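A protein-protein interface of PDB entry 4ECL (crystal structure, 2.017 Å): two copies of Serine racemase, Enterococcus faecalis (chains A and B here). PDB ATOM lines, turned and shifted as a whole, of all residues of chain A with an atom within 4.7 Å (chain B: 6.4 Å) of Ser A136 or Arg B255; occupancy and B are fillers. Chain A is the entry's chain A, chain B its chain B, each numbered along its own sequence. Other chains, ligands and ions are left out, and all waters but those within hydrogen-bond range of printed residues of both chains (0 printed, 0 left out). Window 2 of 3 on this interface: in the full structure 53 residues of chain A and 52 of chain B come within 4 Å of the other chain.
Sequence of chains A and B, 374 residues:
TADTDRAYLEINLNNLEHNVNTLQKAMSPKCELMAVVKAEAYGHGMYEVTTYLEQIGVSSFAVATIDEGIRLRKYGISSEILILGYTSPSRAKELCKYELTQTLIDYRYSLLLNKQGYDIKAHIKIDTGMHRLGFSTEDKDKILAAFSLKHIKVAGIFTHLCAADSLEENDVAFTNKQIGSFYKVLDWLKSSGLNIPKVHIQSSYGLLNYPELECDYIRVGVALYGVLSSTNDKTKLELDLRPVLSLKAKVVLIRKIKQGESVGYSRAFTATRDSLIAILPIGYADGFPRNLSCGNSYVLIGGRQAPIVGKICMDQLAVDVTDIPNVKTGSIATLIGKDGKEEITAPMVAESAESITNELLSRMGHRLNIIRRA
O of Arg B255 lies within hydrogen-bond range of N of Ile B277, at 2.7 Å. OD1 of Asp A127 lies within hydrogen-bond range of N of His A131. The backbone carbonyl oxygen of Leu B253 lies within hydrogen-bond range of the backbone NH of Ile B279. The backbone NH (N) of Asp A127 is in hydrogen-bond range of the backbone carbonyl oxygen (O) of Phe A135.
Ser A136 touches just one residue of chain B: Arg B255. Of chain A, only Asp A127 (3.4 Å), His A131 (3.3 Å), Arg A132 (2.8 Å), Leu A133 (3.6 Å), Gly A134 (2.7 Å) and Ser A136 (3.5 Å) come within 4 Å of Arg B255. Of the printed residues of chain B, Leu A133 touches Arg B255 and Ile B279. Printed residues of chain A within 4 Å of Ile B279: Arg A132 (3.8 Å) and Leu A133 (3.9 Å). Of the printed residues of chain B, Gly A134 touches Arg B255 (2.7 Å). Ile B257 touches none of the printed residues of chain A. Thr A137 touches none of the printed residues of chain B. The nearest residue of chain B that does not touch Ser A136 is Lys B256 (5.9 Å). The nearest printed residue of chain A that does not touch Arg B255 is Phe A135 (5.0 Å).
Printed residues of chain A that touch a printed residue of chain B: Asp A127, His A131, Arg A132, Leu A133, Gly A134 and Ser A136. Hydrophobic or aromatic side chains of chain A that line the printed part of chain B: His A131 and Leu A133. Along chain A the printed residues that touch a printed residue of chain B span positions 127 to 136.
No position is printed for both chains. Of the 10 pairs that touch across the chains among the printed residues, none has its exchanged pair printed and touching as well.
The backbone carbonyl oxygen of His A131 lies close to the guanidinium group of Arg B255 (3.4 Å). O of Arg A132 sits at hydrogen-bond distance from NH2 of Arg B255 (2.8 Å). NH2 of Arg B255 is in hydrogen-bond range of O of Gly A134 (2.7 Å). The guanidinium group of Arg B255 lies within salt-bridge range of the side-chain carboxylate of Asp A127, 3.4 Å away. The side-chain hydroxyl (OG) of Ser A136 lies within hydrogen-bond range of the guanidinium group (NH1) of Arg B255, at 3.5 Å.
Among the printed residues, merely in contact across the chains: Leu A133 with Arg B255, Arg A132 with Leu B253, Arg A132 with Val B263, Arg A132 with Ile B279 and Leu A133 with Ile B279.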
ATOM      1  N   ASP A 127     -27.821  24.700  -8.956  1.00  0.00           N
ATOM      2  CA  ASP A 127     -28.695  25.259  -7.936  1.00  0.00           C
ATOM      3  C   ASP A 127     -29.858  25.940  -8.636  1.00  0.00           C
ATOM      4  O   ASP A 127     -29.657  26.908  -9.379  1.00  0.00           O
ATOM      5  CB  ASP A 127     -27.937  26.258  -7.047  1.00  0.00           C
ATOM      6  CG  ASP A 127     -28.867  27.098  -6.171  1.00  0.00           C
ATOM      7  OD1 ASP A 127     -30.015  26.669  -5.914  1.00  0.00           O
ATOM      8  OD2 ASP A 127     -28.449  28.196  -5.730  1.00  0.00           O
ATOM      9  N   HIS A 131     -30.391  26.987  -3.070  1.00  0.00           N
ATOM     10  CA  HIS A 131     -29.340  27.881  -2.594  1.00  0.00           C
ATOM     11  C   HIS A 131     -28.423  27.240  -1.550  1.00  0.00           C
ATOM     12  O   HIS A 131     -27.960  27.898  -0.617  1.00  0.00           O
ATOM     13  CB  HIS A 131     -29.956  29.164  -2.046  1.00  0.00           C
ATOM     14  CG  HIS A 131     -30.698  29.953  -3.077  1.00  0.00           C
ATOM     15  ND1 HIS A 131     -31.720  30.823  -2.761  1.00  0.00           N
ATOM     16  CD2 HIS A 131     -30.573  29.991  -4.425  1.00  0.00           C
ATOM     17  CE1 HIS A 131     -32.189  31.367  -3.870  1.00  0.00           C
ATOM     18  NE2 HIS A 131     -31.505  30.884  -4.893  1.00  0.00           N
ATOM     19  N   ARG A 132     -28.145  25.959  -1.724  1.00  0.00           N
ATOM     20  CA  ARG A 132     -27.115  25.303  -0.945  1.00  0.00           C
ATOM     21  C   ARG A 132     -25.961  24.967  -1.884  1.00  0.00           C
ATOM     22  O   ARG A 132     -25.141  25.832  -2.182  1.00  0.00           O
ATOM     23  CB  ARG A 132     -27.663  24.066  -0.215  1.00  0.00           C
ATOM     24  CG  ARG A 132     -28.760  24.404   0.810  1.00  0.00           C
ATOM     25  CD  ARG A 132     -29.318  23.155   1.558  1.00  0.00           C
ATOM     26  NE  ARG A 132     -30.533  23.502   2.303  1.00  0.00           N
ATOM     27  CZ  ARG A 132     -30.546  23.987   3.546  1.00  0.00           C
ATOM     28  NH1 ARG A 132     -29.410  24.148   4.217  1.00  0.00           N
ATOM     29  NH2 ARG A 132     -31.699  24.297   4.132  1.00  0.00           N
ATOM     30  N   LEU A 133     -25.891  23.728  -2.353  1.00  0.00           N
ATOM     31  CA  LEU A 133     -24.839  23.358  -3.289  1.00  0.00           C
ATOM     32  C   LEU A 133     -25.306  23.575  -4.724  1.00  0.00           C
ATOM     33  O   LEU A 133     -26.515  23.614  -4.989  1.00  0.00           O
ATOM     34  CB  LEU A 133     -24.428  21.903  -3.111  1.00  0.00           C
ATOM     35  CG  LEU A 133     -24.097  21.397  -1.703  1.00  0.00           C
ATOM     36  CD1 LEU A 133     -24.130  19.844  -1.707  1.00  0.00           C
ATOM     37  CD2 LEU A 133     -22.774  21.889  -1.235  1.00  0.00           C
ATOM     38  N   GLY A 134     -24.344  23.720  -5.640  1.00  0.00           N
ATOM     39  CA  GLY A 134     -24.645  23.771  -7.059  1.00  0.00           C
ATOM     40  C   GLY A 134     -24.214  25.057  -7.736  1.00  0.00           C
ATOM     41  O   GLY A 134     -24.099  26.108  -7.093  1.00  0.00           O
ATOM     42  N   PHE A 135     -23.965  24.952  -9.043  1.00  0.00           N
ATOM     43  CA  PHE A 135     -23.689  26.095  -9.913  1.00  0.00           C
ATOM     44  C   PHE A 135     -24.951  26.944 -10.024  1.00  0.00           C
ATOM     45  O   PHE A 135     -26.041  26.403 -10.148  1.00  0.00           O
ATOM     46  CB  PHE A 135     -23.352  25.602 -11.320  1.00  0.00           C
ATOM     47  CG  PHE A 135     -21.989  24.980 -11.461  1.00  0.00           C
ATOM     48  CD1 PHE A 135     -21.637  23.853 -10.741  1.00  0.00           C
ATOM     49  CD2 PHE A 135     -21.067  25.507 -12.367  1.00  0.00           C
ATOM     50  CE1 PHE A 135     -20.389  23.268 -10.894  1.00  0.00           C
ATOM     51  CE2 PHE A 135     -19.813  24.927 -12.531  1.00  0.00           C
ATOM     52  CZ  PHE A 135     -19.472  23.804 -11.794  1.00  0.00           C
ATOM     53  N   SER A 136     -24.815  28.267 -10.022  1.00  0.00           N
ATOM     54  CA  SER A 136     -25.976  29.146 -10.163  1.00  0.00           C
ATOM     55  C   SER A 136     -26.489  29.133 -11.596  1.00  0.00           C
ATOM     56  O   SER A 136     -25.735  28.864 -12.523  1.00  0.00           O
ATOM     57  CB  SER A 136     -25.632  30.571  -9.735  1.00  0.00           C
ATOM     58  OG  SER A 136     -25.344  30.608  -8.345  1.00  0.00           O
ATOM     59  N   THR A 137     -27.775  29.408 -11.777  1.00  0.00           N
ATOM     60  CA  THR A 137     -28.357  29.397 -13.113  1.00  0.00           C
ATOM     61  C   THR A 137     -27.893  30.602 -13.922  1.00  0.00           C
ATOM     62  O   THR A 137     -27.970  30.588 -15.148  1.00  0.00           O
ATOM     63  CB  THR A 137     -29.893  29.376 -13.083  1.00  0.00           C
ATOM     64  OG1 THR A 137     -30.371  30.430 -12.239  1.00  0.00           O
ATOM     65  CG2 THR A 137     -30.399  28.045 -12.567  1.00  0.00           C
ATOM     66  N   GLU A 138     -27.423  31.639 -13.233  1.00  0.00           N
ATOM     67  CA  GLU A 138     -26.892  32.821 -13.906  1.00  0.00           C
ATOM     68  C   GLU A 138     -25.627  32.431 -14.638  1.00  0.00           C
ATOM     69  O   GLU A 138     -25.512  32.623 -15.843  1.00  0.00           O
ATOM     70  CB  GLU A 138     -26.540  33.918 -12.903  1.00  0.00           C
ATOM     71  CG  GLU A 138     -27.326  33.888 -11.613  1.00  0.00           C
ATOM     72  CD  GLU A 138     -28.596  34.705 -11.688  1.00  0.00           C
ATOM     73  OE1 GLU A 138     -29.263  34.664 -12.744  1.00  0.00           O
ATOM     74  OE2 GLU A 138     -28.920  35.395 -10.694  1.00  0.00           O
ATOM     75  N   ASP A 139     -24.697  31.845 -13.894  1.00  0.00           N
ATOM     76  CA  ASP A 139     -23.334  31.624 -14.361  1.00  0.00           C
ATOM     77  C   ASP A 139     -23.235  30.545 -15.434  1.00  0.00           C
ATOM     78  O   ASP A 139     -22.494  29.571 -15.278  1.00  0.00           O
ATOM     79  CB  ASP A 139     -22.416  31.290 -13.174  1.00  0.00           C
ATOM     80  CG  ASP A 139     -22.591  32.259 -12.001  1.00  0.00           C
ATOM     81  OD1 ASP A 139     -23.063  33.394 -12.224  1.00  0.00           O
ATOM     82  OD2 ASP A 139     -22.256  31.883 -10.853  1.00  0.00           O
ATOM     83  N   ILE A 143     -20.755  26.816 -15.996  1.00  0.00           N
ATOM     84  CA  ILE A 143     -21.311  25.479 -16.199  1.00  0.00           C
ATOM     85  C   ILE A 143     -20.736  24.828 -17.458  1.00  0.00           C
ATOM     86  O   ILE A 143     -20.271  23.682 -17.431  1.00  0.00           O
ATOM     87  CB  ILE A 143     -22.851  25.519 -16.286  1.00  0.00           C
ATOM     88  CG1 ILE A 143     -23.440  25.969 -14.944  1.00  0.00           C
ATOM     89  CG2 ILE A 143     -23.412  24.136 -16.672  1.00  0.00           C
ATOM     90  CD1 ILE A 143     -24.886  26.436 -15.025  1.00  0.00           C
ATOM     91  N   LEU B 253     -18.489  25.443   0.695  1.00  0.00           N
ATOM     92  CA  LEU B 253     -18.936  26.292  -0.419  1.00  0.00           C
ATOM     93  C   LEU B 253     -19.498  27.568   0.156  1.00  0.00           C
ATOM     94  O   LEU B 253     -20.105  27.568   1.240  1.00  0.00           O
ATOM     95  CB  LEU B 253     -20.013  25.589  -1.262  1.00  0.00           C
ATOM     96  CG  LEU B 253     -20.660  26.288  -2.480  1.00  0.00           C
ATOM     97  CD1 LEU B 253     -21.158  25.227  -3.442  1.00  0.00           C
ATOM     98  CD2 LEU B 253     -21.842  27.161  -2.090  1.00  0.00           C
ATOM     99  N   ILE B 254     -19.267  28.664  -0.551  1.00  0.00           N
ATOM    100  CA  ILE B 254     -19.817  29.944  -0.164  1.00  0.00           C
ATOM    101  C   ILE B 254     -20.619  30.495  -1.337  1.00  0.00           C
ATOM    102  O   ILE B 254     -20.231  30.331  -2.491  1.00  0.00           O
ATOM    103  CB  ILE B 254     -18.702  30.934   0.230  1.00  0.00           C
ATOM    104  CG1 ILE B 254     -17.933  30.416   1.456  1.00  0.00           C
ATOM    105  CG2 ILE B 254     -19.288  32.294   0.509  1.00  0.00           C
ATOM    106  CD1 ILE B 254     -16.757  31.300   1.879  1.00  0.00           C
ATOM    107  N   ARG B 255     -21.754  31.116  -1.051  1.00  0.00           N
ATOM    108  CA  ARG B 255     -22.563  31.687  -2.108  1.00  0.00           C
ATOM    109  C   ARG B 255     -23.211  32.981  -1.653  1.00  0.00           C
ATOM    110  O   ARG B 255     -23.395  33.213  -0.454  1.00  0.00           O
ATOM    111  CB  ARG B 255     -23.631  30.694  -2.603  1.00  0.00           C
ATOM    112  CG  ARG B 255     -24.884  30.552  -1.724  1.00  0.00           C
ATOM    113  CD  ARG B 255     -26.036  29.794  -2.454  1.00  0.00           C
ATOM    114  NE  ARG B 255     -25.595  28.501  -2.982  1.00  0.00           N
ATOM    115  CZ  ARG B 255     -25.236  28.290  -4.249  1.00  0.00           C
ATOM    116  NH1 ARG B 255     -25.281  29.286  -5.133  1.00  0.00           N
ATOM    117  NH2 ARG B 255     -24.817  27.091  -4.634  1.00  0.00           N
ATOM    118  N   LYS B 256     -23.542  33.826  -2.624  1.00  0.00           N
ATOM    119  CA  LYS B 256     -24.286  35.038  -2.360  1.00  0.00           C
ATOM    120  C   LYS B 256     -25.745  34.744  -2.623  1.00  0.00           C
ATOM    121  O   LYS B 256     -26.086  34.079  -3.597  1.00  0.00           O
ATOM    122  CB  LYS B 256     -23.816  36.165  -3.297  1.00  0.00           C
ATOM    123  CG  LYS B 256     -24.523  37.499  -3.086  1.00  0.00           C
ATOM    124  CD  LYS B 256     -23.933  38.610  -3.977  1.00  0.00           C
ATOM    125  CE  LYS B 256     -22.484  38.951  -3.603  1.00  0.00           C
ATOM    126  NZ  LYS B 256     -21.492  38.631  -4.687  1.00  0.00           N
ATOM    127  N   ILE B 257     -26.613  35.233  -1.752  1.00  0.00           N
ATOM    128  CA  ILE B 257     -28.031  35.256  -2.073  1.00  0.00           C
ATOM    129  C   ILE B 257     -28.522  36.689  -1.992  1.00  0.00           C
ATOM    130  O   ILE B 257     -28.060  37.482  -1.158  1.00  0.00           O
ATOM    131  CB  ILE B 257     -28.880  34.358  -1.145  1.00  0.00           C
ATOM    132  CG1 ILE B 257     -28.814  34.854   0.301  1.00  0.00           C
ATOM    133  CG2 ILE B 257     -28.466  32.877  -1.269  1.00  0.00           C
ATOM    134  CD1 ILE B 257     -29.644  34.025   1.252  1.00  0.00           C
ATOM    135  N   VAL B 263     -33.149  30.127   1.898  1.00  0.00           N
ATOM    136  CA  VAL B 263     -32.366  28.913   1.723  1.00  0.00           C
ATOM    137  C   VAL B 263     -33.273  27.708   1.963  1.00  0.00           C
ATOM    138  O   VAL B 263     -33.913  27.597   3.007  1.00  0.00           O
ATOM    139  CB  VAL B 263     -31.147  28.871   2.658  1.00  0.00           C
ATOM    140  CG1 VAL B 263     -30.424  27.531   2.534  1.00  0.00           C
ATOM    141  CG2 VAL B 263     -30.201  30.018   2.325  1.00  0.00           C
ATOM    142  N   SER B 275     -26.853  38.590   1.140  1.00  0.00           N
ATOM    143  CA  SER B 275     -26.161  37.832   2.174  1.00  0.00           C
ATOM    144  C   SER B 275     -25.179  36.827   1.605  1.00  0.00           C
ATOM    145  O   SER B 275     -25.341  36.336   0.485  1.00  0.00           O
ATOM    146  CB  SER B 275     -27.169  37.100   3.065  1.00  0.00           C
ATOM    147  OG  SER B 275     -28.122  37.994   3.602  1.00  0.00           O
ATOM    148  N   LEU B 276     -24.166  36.514   2.397  1.00  0.00           N
ATOM    149  CA  LEU B 276     -23.187  35.513   2.014  1.00  0.00           C
ATOM    150  C   LEU B 276     -23.426  34.285   2.871  1.00  0.00           C
ATOM    151  O   LEU B 276     -23.419  34.358   4.101  1.00  0.00           O
ATOM    152  CB  LEU B 276     -21.762  36.036   2.206  1.00  0.00           C
ATOM    153  CG  LEU B 276     -21.217  36.905   1.067  1.00  0.00           C
ATOM    154  CD1 LEU B 276     -21.211  36.129  -0.250  1.00  0.00           C
ATOM    155  CD2 LEU B 276     -21.993  38.204   0.937  1.00  0.00           C
ATOM    156  N   ILE B 277     -23.657  33.157   2.218  1.00  0.00           N
ATOM    157  CA  ILE B 277     -24.007  31.933   2.926  1.00  0.00           C
ATOM    158  C   ILE B 277     -22.864  30.942   2.837  1.00  0.00           C
ATOM    159  O   ILE B 277     -22.309  30.729   1.765  1.00  0.00           O
ATOM    160  CB  ILE B 277     -25.273  31.292   2.308  1.00  0.00           C
ATOM    161  CG1 ILE B 277     -26.466  32.239   2.436  1.00  0.00           C
ATOM    162  CG2 ILE B 277     -25.589  29.958   2.963  1.00  0.00           C
ATOM    163  CD1 ILE B 277     -26.705  32.731   3.852  1.00  0.00           C
ATOM    164  N   ALA B 278     -22.516  30.323   3.958  1.00  0.00           N
ATOM    165  CA  ALA B 278     -21.551  29.235   3.934  1.00  0.00           C
ATOM    166  C   ALA B 278     -22.248  27.890   4.144  1.00  0.00           C
ATOM    167  O   ALA B 278     -23.136  27.754   4.997  1.00  0.00           O
ATOM    168  CB  ALA B 278     -20.489  29.445   4.986  1.00  0.00           C
ATOM    169  N   ILE B 279     -21.830  26.892   3.374  1.00  0.00           N
ATOM    170  CA  ILE B 279     -22.379  25.556   3.502  1.00  0.00           C
ATOM    171  C   ILE B 279     -21.448  24.682   4.329  1.00  0.00           C
ATOM    172  O   ILE B 279     -20.246  24.601   4.031  1.00  0.00           O
ATOM    173  CB  ILE B 279     -22.590  24.913   2.129  1.00  0.00           C
ATOM    174  CG1 ILE B 279     -23.473  25.818   1.267  1.00  0.00           C
ATOM    175  CG2 ILE B 279     -23.192  23.518   2.282  1.00  0.00           C
ATOM    176  CD1 ILE B 279     -24.758  26.249   1.967  1.00  0.00           C
